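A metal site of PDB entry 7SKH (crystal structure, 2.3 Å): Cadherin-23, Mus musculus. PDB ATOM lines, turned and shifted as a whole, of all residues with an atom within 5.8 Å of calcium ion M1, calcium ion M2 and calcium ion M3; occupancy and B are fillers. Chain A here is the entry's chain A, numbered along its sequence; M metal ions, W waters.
Four residues have an atom within 4 Å of calcium ion M1: Glu 17, Asp 71, Glu 73 and Asp 111.
The nearest printed residue that does not touch calcium ion M1 is Tyr 72 (4.2 Å).
The side-chain carboxylate (OE1) of Glu 73 is bound to calcium ion M1, at 2.2 Å.
Calcium ion M1 is bound by OD1 of Asp 71, 2.2 Å away.
The side-chain carboxylate (OE2) of Glu 17 is bound to calcium ion M1, at 2.3 Å.
Calcium ion M1 is bound by OD2 of Asp 111.
Water W2 is bound to calcium ion M1 (2.4 Å).
Calcium ion M1 is bound by water W1 (2.6 Å).
N of Asp 197 is in hydrogen-bond range of O of Leu 203, at 2.9 Å.
OD1 of Asn 112 sits at hydrogen-bond distance from NH1 of Arg 143, 2.7 Å away.
The side-chain carboxylate of Glu 73 lies close to the side-chain amide nitrogen of Asn 112, 3.2 Å away.
The side-chain carboxylate (OD1) of Asp 111 sits close to the side-chain amide nitrogen (ND2) of Asn 112 (3.1 Å).
The backbone NH (N) of Tyr 72 lies close to the side-chain carboxylate (OE2) of Glu 17 (2.8 Å).
OD2 of Asp 108 sits at hydrogen-bond distance from ND2 of Asn 148.
OD2 of Asp 108 lies within hydrogen-bond range of N of Ser 145.
Water W2 bridges ND2 of Asn 112 (3.1 Å) and NH1 of Arg 143 (3.3 Å).
Of the 21 residues printed, 7 come within 4 Å of calcium ion M2.
The nearest printed residue that does not touch calcium ion M2 is Tyr 72 (4.5 Å).
Calcium ion M2 is bound by OD1 of Asp 108 (2.3 Å), OD1 of Asp 111 (2.3 Å), OE1 of Glu 17 (2.3 Å), OE2 of Glu 73 (2.4 Å), O of Ile 109 (2.4 Å), OD1 of Asp 144 (2.5 Å) and OE1 of Glu 73 (2.7 Å).
Calcium ion M3 is bound by the backbone carbonyl oxygen (O) of Asn 112 (2.3 Å), the side-chain carboxylate (OD2) of Asp 144 (2.3 Å), the side-chain amide oxygen (OD1) of Asn 110 (2.3 Å), the backbone carbonyl oxygen (O) of Asn 148 (2.4 Å), the side-chain carboxylate (OD2) of Asp 197 (2.4 Å), the side-chain carboxylate (OD2) of Asp 142 (2.4 Å) and the side-chain carboxylate (OD1) of Asp 142 (2.6 Å).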
ATOM      1  N   GLU A  17     -25.123   2.268   8.672  1.00  0.00           N
ATOM      2  CA  GLU A  17     -25.561   1.352   7.607  1.00  0.00           C
ATOM      3  C   GLU A  17     -24.467   0.293   7.414  1.00  0.00           C
ATOM      4  O   GLU A  17     -23.369   0.477   7.943  1.00  0.00           O
ATOM      5  CB  GLU A  17     -25.793   2.109   6.307  1.00  0.00           C
ATOM      6  CG  GLU A  17     -24.506   2.529   5.627  1.00  0.00           C
ATOM      7  CD  GLU A  17     -24.731   3.038   4.221  1.00  0.00           C
ATOM      8  OE1 GLU A  17     -23.977   3.968   3.793  1.00  0.00           O
ATOM      9  OE2 GLU A  17     -25.654   2.497   3.536  1.00  0.00           O
ATOM     10  N   GLU A  69     -30.045  -5.531   5.022  1.00  0.00           N
ATOM     11  CA  GLU A  69     -28.998  -4.545   5.327  1.00  0.00           C
ATOM     12  C   GLU A  69     -29.632  -3.148   5.464  1.00  0.00           C
ATOM     13  O   GLU A  69     -30.402  -2.729   4.598  1.00  0.00           O
ATOM     14  CB  GLU A  69     -27.969  -4.658   4.211  1.00  0.00           C
ATOM     15  CG  GLU A  69     -26.750  -3.845   4.479  1.00  0.00           C
ATOM     16  CD  GLU A  69     -25.789  -3.865   3.323  1.00  0.00           C
ATOM     17  OE1 GLU A  69     -25.811  -4.864   2.605  1.00  0.00           O
ATOM     18  OE2 GLU A  69     -25.044  -2.868   3.157  1.00  0.00           O
ATOM     19  N   LEU A  70     -29.345  -2.456   6.554  1.00  0.00           N
ATOM     20  CA  LEU A  70     -29.669  -1.018   6.688  1.00  0.00           C
ATOM     21  C   LEU A  70     -28.826  -0.290   5.671  1.00  0.00           C
ATOM     22  O   LEU A  70     -27.635  -0.596   5.561  1.00  0.00           O
ATOM     23  CB  LEU A  70     -29.340  -0.575   8.103  1.00  0.00           C
ATOM     24  CG  LEU A  70     -30.222  -1.179   9.195  1.00  0.00           C
ATOM     25  CD1 LEU A  70     -30.146  -0.342  10.458  1.00  0.00           C
ATOM     26  CD2 LEU A  70     -31.664  -1.279   8.722  1.00  0.00           C
ATOM     27  N   ASP A  71     -29.424   0.619   4.951  1.00  0.00           N
ATOM     28  CA  ASP A  71     -28.826   1.234   3.747  1.00  0.00           C
ATOM     29  C   ASP A  71     -29.181   2.712   3.796  1.00  0.00           C
ATOM     30  O   ASP A  71     -30.380   3.051   3.703  1.00  0.00           O
ATOM     31  CB  ASP A  71     -29.346   0.593   2.462  1.00  0.00           C
ATOM     32  CG  ASP A  71     -28.717   1.160   1.196  1.00  0.00           C
ATOM     33  OD1 ASP A  71     -27.640   1.819   1.315  1.00  0.00           O
ATOM     34  OD2 ASP A  71     -29.293   0.974   0.116  1.00  0.00           O
ATOM     35  N   TYR A  72     -28.161   3.553   3.944  1.00  0.00           N
ATOM     36  CA  TYR A  72     -28.333   5.019   3.894  1.00  0.00           C
ATOM     37  C   TYR A  72     -28.902   5.415   2.536  1.00  0.00           C
ATOM     38  O   TYR A  72     -29.646   6.378   2.496  1.00  0.00           O
ATOM     39  CB  TYR A  72     -27.010   5.728   4.167  1.00  0.00           C
ATOM     40  CG  TYR A  72     -27.169   7.214   4.361  1.00  0.00           C
ATOM     41  CD1 TYR A  72     -27.184   8.056   3.272  1.00  0.00           C
ATOM     42  CD2 TYR A  72     -27.304   7.768   5.625  1.00  0.00           C
ATOM     43  CE1 TYR A  72     -27.302   9.427   3.432  1.00  0.00           C
ATOM     44  CE2 TYR A  72     -27.457   9.133   5.805  1.00  0.00           C
ATOM     45  CZ  TYR A  72     -27.440   9.964   4.705  1.00  0.00           C
ATOM     46  OH  TYR A  72     -27.579  11.322   4.810  1.00  0.00           O
ATOM     47  N   GLU A  73     -28.526   4.724   1.457  1.00  0.00           N
ATOM     48  CA  GLU A  73     -28.876   5.174   0.096  1.00  0.00           C
ATOM     49  C   GLU A  73     -30.359   4.914  -0.172  1.00  0.00           C
ATOM     50  O   GLU A  73     -30.916   5.599  -1.006  1.00  0.00           O
ATOM     51  CB  GLU A  73     -27.963   4.527  -0.948  1.00  0.00           C
ATOM     52  CG  GLU A  73     -26.575   5.142  -1.015  1.00  0.00           C
ATOM     53  CD  GLU A  73     -25.669   4.997   0.209  1.00  0.00           C
ATOM     54  OE1 GLU A  73     -25.411   3.894   0.642  1.00  0.00           O
ATOM     55  OE2 GLU A  73     -25.149   6.003   0.699  1.00  0.00           O
ATOM     56  N   ASP A 108     -24.294   7.411   7.054  1.00  0.00           N
ATOM     57  CA  ASP A 108     -23.693   7.115   5.732  1.00  0.00           C
ATOM     58  C   ASP A 108     -22.271   6.562   5.921  1.00  0.00           C
ATOM     59  O   ASP A 108     -21.531   7.151   6.664  1.00  0.00           O
ATOM     60  CB  ASP A 108     -23.690   8.362   4.865  1.00  0.00           C
ATOM     61  CG  ASP A 108     -23.283   8.133   3.415  1.00  0.00           C
ATOM     62  OD1 ASP A 108     -23.505   7.015   2.888  1.00  0.00           O
ATOM     63  OD2 ASP A 108     -22.778   9.094   2.812  1.00  0.00           O
ATOM     64  N   ILE A 109     -21.945   5.414   5.310  1.00  0.00           N
ATOM     65  CA  ILE A 109     -20.526   4.950   5.140  1.00  0.00           C
ATOM     66  C   ILE A 109     -20.186   4.989   3.638  1.00  0.00           C
ATOM     67  O   ILE A 109     -21.107   4.952   2.785  1.00  0.00           O
ATOM     68  CB  ILE A 109     -20.284   3.551   5.764  1.00  0.00           C
ATOM     69  CG1 ILE A 109     -20.831   2.402   4.921  1.00  0.00           C
ATOM     70  CG2 ILE A 109     -20.815   3.495   7.196  1.00  0.00           C
ATOM     71  CD1 ILE A 109     -20.559   0.996   5.497  1.00  0.00           C
ATOM     72  N   ASN A 110     -18.897   5.016   3.342  1.00  0.00           N
ATOM     73  CA  ASN A 110     -18.386   5.078   1.961  1.00  0.00           C
ATOM     74  C   ASN A 110     -18.470   3.659   1.378  1.00  0.00           C
ATOM     75  O   ASN A 110     -17.442   2.948   1.400  1.00  0.00           O
ATOM     76  CB  ASN A 110     -16.991   5.688   1.909  1.00  0.00           C
ATOM     77  CG  ASN A 110     -16.649   6.119   0.506  1.00  0.00           C
ATOM     78  OD1 ASN A 110     -17.533   6.520  -0.254  1.00  0.00           O
ATOM     79  ND2 ASN A 110     -15.365   6.104   0.174  1.00  0.00           N
ATOM     80  N   ASP A 111     -19.652   3.266   0.902  1.00  0.00           N
ATOM     81  CA  ASP A 111     -19.891   1.928   0.294  1.00  0.00           C
ATOM     82  C   ASP A 111     -20.284   2.061  -1.190  1.00  0.00           C
ATOM     83  O   ASP A 111     -20.720   1.044  -1.741  1.00  0.00           O
ATOM     84  CB  ASP A 111     -20.920   1.109   1.097  1.00  0.00           C
ATOM     85  CG  ASP A 111     -22.292   1.758   1.290  1.00  0.00           C
ATOM     86  OD1 ASP A 111     -22.433   2.982   1.020  1.00  0.00           O
ATOM     87  OD2 ASP A 111     -23.214   1.040   1.701  1.00  0.00           O
ATOM     88  N   ASN A 112     -20.169   3.237  -1.828  1.00  0.00           N
ATOM     89  CA  ASN A 112     -20.434   3.412  -3.278  1.00  0.00           C
ATOM     90  C   ASN A 112     -19.172   3.995  -3.936  1.00  0.00           C
ATOM     91  O   ASN A 112     -18.618   4.999  -3.416  1.00  0.00           O
ATOM     92  CB  ASN A 112     -21.715   4.211  -3.541  1.00  0.00           C
ATOM     93  CG  ASN A 112     -22.946   3.439  -3.087  1.00  0.00           C
ATOM     94  OD1 ASN A 112     -23.473   2.632  -3.835  1.00  0.00           O
ATOM     95  ND2 ASN A 112     -23.363   3.629  -1.848  1.00  0.00           N
ATOM     96  N   VAL A 113     -18.709   3.325  -4.989  1.00  0.00           N
ATOM     97  CA  VAL A 113     -17.544   3.719  -5.826  1.00  0.00           C
ATOM     98  C   VAL A 113     -18.013   4.818  -6.776  1.00  0.00           C
ATOM     99  O   VAL A 113     -19.101   4.696  -7.337  1.00  0.00           O
ATOM    100  CB  VAL A 113     -17.031   2.503  -6.621  1.00  0.00           C
ATOM    101  CG1 VAL A 113     -15.772   2.838  -7.388  1.00  0.00           C
ATOM    102  CG2 VAL A 113     -16.799   1.278  -5.748  1.00  0.00           C
ATOM    103  N   PRO A 114     -17.238   5.916  -6.958  1.00  0.00           N
ATOM    104  CA  PRO A 114     -17.578   6.922  -7.962  1.00  0.00           C
ATOM    105  C   PRO A 114     -17.464   6.224  -9.313  1.00  0.00           C
ATOM    106  O   PRO A 114     -16.407   5.713  -9.577  1.00  0.00           O
ATOM    107  CB  PRO A 114     -16.535   8.022  -7.810  1.00  0.00           C
ATOM    108  CG  PRO A 114     -15.426   7.421  -6.948  1.00  0.00           C
ATOM    109  CD  PRO A 114     -16.011   6.243  -6.219  1.00  0.00           C
ATOM    110  N   ASP A 142     -21.511   9.320  -7.709  1.00  0.00           N
ATOM    111  CA  ASP A 142     -21.284   8.630  -6.413  1.00  0.00           C
ATOM    112  C   ASP A 142     -22.590   8.670  -5.616  1.00  0.00           C
ATOM    113  O   ASP A 142     -23.013   9.744  -5.246  1.00  0.00           O
ATOM    114  CB  ASP A 142     -20.087   9.258  -5.693  1.00  0.00           C
ATOM    115  CG  ASP A 142     -19.566   8.378  -4.587  1.00  0.00           C
ATOM    116  OD1 ASP A 142     -20.387   7.955  -3.743  1.00  0.00           O
ATOM    117  OD2 ASP A 142     -18.357   8.122  -4.572  1.00  0.00           O
ATOM    118  N   ARG A 143     -23.150   7.516  -5.298  1.00  0.00           N
ATOM    119  CA  ARG A 143     -24.486   7.381  -4.653  1.00  0.00           C
ATOM    120  C   ARG A 143     -24.415   7.814  -3.184  1.00  0.00           C
ATOM    121  O   ARG A 143     -25.471   8.028  -2.610  1.00  0.00           O
ATOM    122  CB  ARG A 143     -24.986   5.931  -4.762  1.00  0.00           C
ATOM    123  CG  ARG A 143     -25.586   5.580  -6.126  1.00  0.00           C
ATOM    124  CD  ARG A 143     -25.841   4.083  -6.294  1.00  0.00           C
ATOM    125  NE  ARG A 143     -27.097   3.652  -5.671  1.00  0.00           N
ATOM    126  CZ  ARG A 143     -27.195   2.993  -4.527  1.00  0.00           C
ATOM    127  NH1 ARG A 143     -26.126   2.629  -3.858  1.00  0.00           N
ATOM    128  NH2 ARG A 143     -28.382   2.685  -4.062  1.00  0.00           N
ATOM    129  N   ASP A 144     -23.213   7.889  -2.590  1.00  0.00           N
ATOM    130  CA  ASP A 144     -23.058   8.339  -1.174  1.00  0.00           C
ATOM    131  C   ASP A 144     -23.336   9.831  -1.050  1.00  0.00           C
ATOM    132  O   ASP A 144     -23.529  10.501  -2.065  1.00  0.00           O
ATOM    133  CB  ASP A 144     -21.661   8.007  -0.602  1.00  0.00           C
ATOM    134  CG  ASP A 144     -21.308   6.533  -0.689  1.00  0.00           C
ATOM    135  OD1 ASP A 144     -22.110   5.723  -0.242  1.00  0.00           O
ATOM    136  OD2 ASP A 144     -20.252   6.216  -1.242  1.00  0.00           O
ATOM    137  N   SER A 145     -23.409  10.305   0.188  1.00  0.00           N
ATOM    138  CA  SER A 145     -23.653  11.709   0.572  1.00  0.00           C
ATOM    139  C   SER A 145     -22.429  12.291   1.298  1.00  0.00           C
ATOM    140  O   SER A 145     -21.493  11.541   1.613  1.00  0.00           O
ATOM    141  CB  SER A 145     -24.895  11.800   1.422  1.00  0.00           C
ATOM    142  OG  SER A 145     -26.001  11.439   0.631  1.00  0.00           O
ATOM    143  N   ASN A 148     -18.232  11.476   1.296  1.00  0.00           N
ATOM    144  CA  ASN A 148     -18.319  10.094   0.785  1.00  0.00           C
ATOM    145  C   ASN A 148     -18.818  10.153  -0.656  1.00  0.00           C
ATOM    146  O   ASN A 148     -18.509   9.273  -1.415  1.00  0.00           O
ATOM    147  CB  ASN A 148     -19.248   9.238   1.636  1.00  0.00           C
ATOM    148  CG  ASN A 148     -18.723   8.872   3.017  1.00  0.00           C
ATOM    149  OD1 ASN A 148     -17.528   8.826   3.261  1.00  0.00           O
ATOM    150  ND2 ASN A 148     -19.648   8.514   3.888  1.00  0.00           N
ATOM    151  N   GLY A 149     -19.611  11.164  -0.994  1.00  0.00           N
ATOM    152  CA  GLY A 149     -20.198  11.337  -2.327  1.00  0.00           C
ATOM    153  C   GLY A 149     -19.513  12.364  -3.187  1.00  0.00           C
ATOM    154  O   GLY A 149     -19.997  12.556  -4.318  1.00  0.00           O
ATOM    155  N   ASP A 197     -13.400   9.559  -4.565  1.00  0.00           N
ATOM    156  CA  ASP A 197     -14.312  10.250  -3.614  1.00  0.00           C
ATOM    157  C   ASP A 197     -13.497  10.728  -2.420  1.00  0.00           C
ATOM    158  O   ASP A 197     -12.306  10.461  -2.367  1.00  0.00           O
ATOM    159  CB  ASP A 197     -15.522   9.386  -3.289  1.00  0.00           C
ATOM    160  CG  ASP A 197     -15.199   8.141  -2.516  1.00  0.00           C
ATOM    161  OD1 ASP A 197     -14.168   8.143  -1.809  1.00  0.00           O
ATOM    162  OD2 ASP A 197     -15.995   7.202  -2.584  1.00  0.00           O
ATOM    163  N   LEU A 203     -12.725   5.581  -2.279  1.00  0.00           N
ATOM    164  CA  LEU A 203     -12.991   4.636  -3.391  1.00  0.00           C
ATOM    165  C   LEU A 203     -12.782   5.412  -4.692  1.00  0.00           C
ATOM    166  O   LEU A 203     -13.086   6.653  -4.713  1.00  0.00           O
ATOM    167  CB  LEU A 203     -14.396   4.059  -3.278  1.00  0.00           C
ATOM    168  CG  LEU A 203     -14.711   3.216  -2.028  1.00  0.00           C
ATOM    169  CD1 LEU A 203     -16.201   2.976  -1.905  1.00  0.00           C
ATOM    170  CD2 LEU A 203     -13.949   1.894  -2.021  1.00  0.00           C
HETATM  171 CA    CA M   1     -25.395   1.779   1.371  1.00  0.00          CA
HETATM  172 CA    CA M   2     -23.295   5.007   1.800  1.00  0.00          CA
HETATM  173 CA    CA M   3     -18.389   7.066  -2.364  1.00  0.00          CA
HETATM  174  O   HOH W   1     -26.049  -0.600   2.058  1.00  0.00           O
HETATM  175  O   HOH W   2     -25.185   1.340  -0.976  1.00  0.00           O
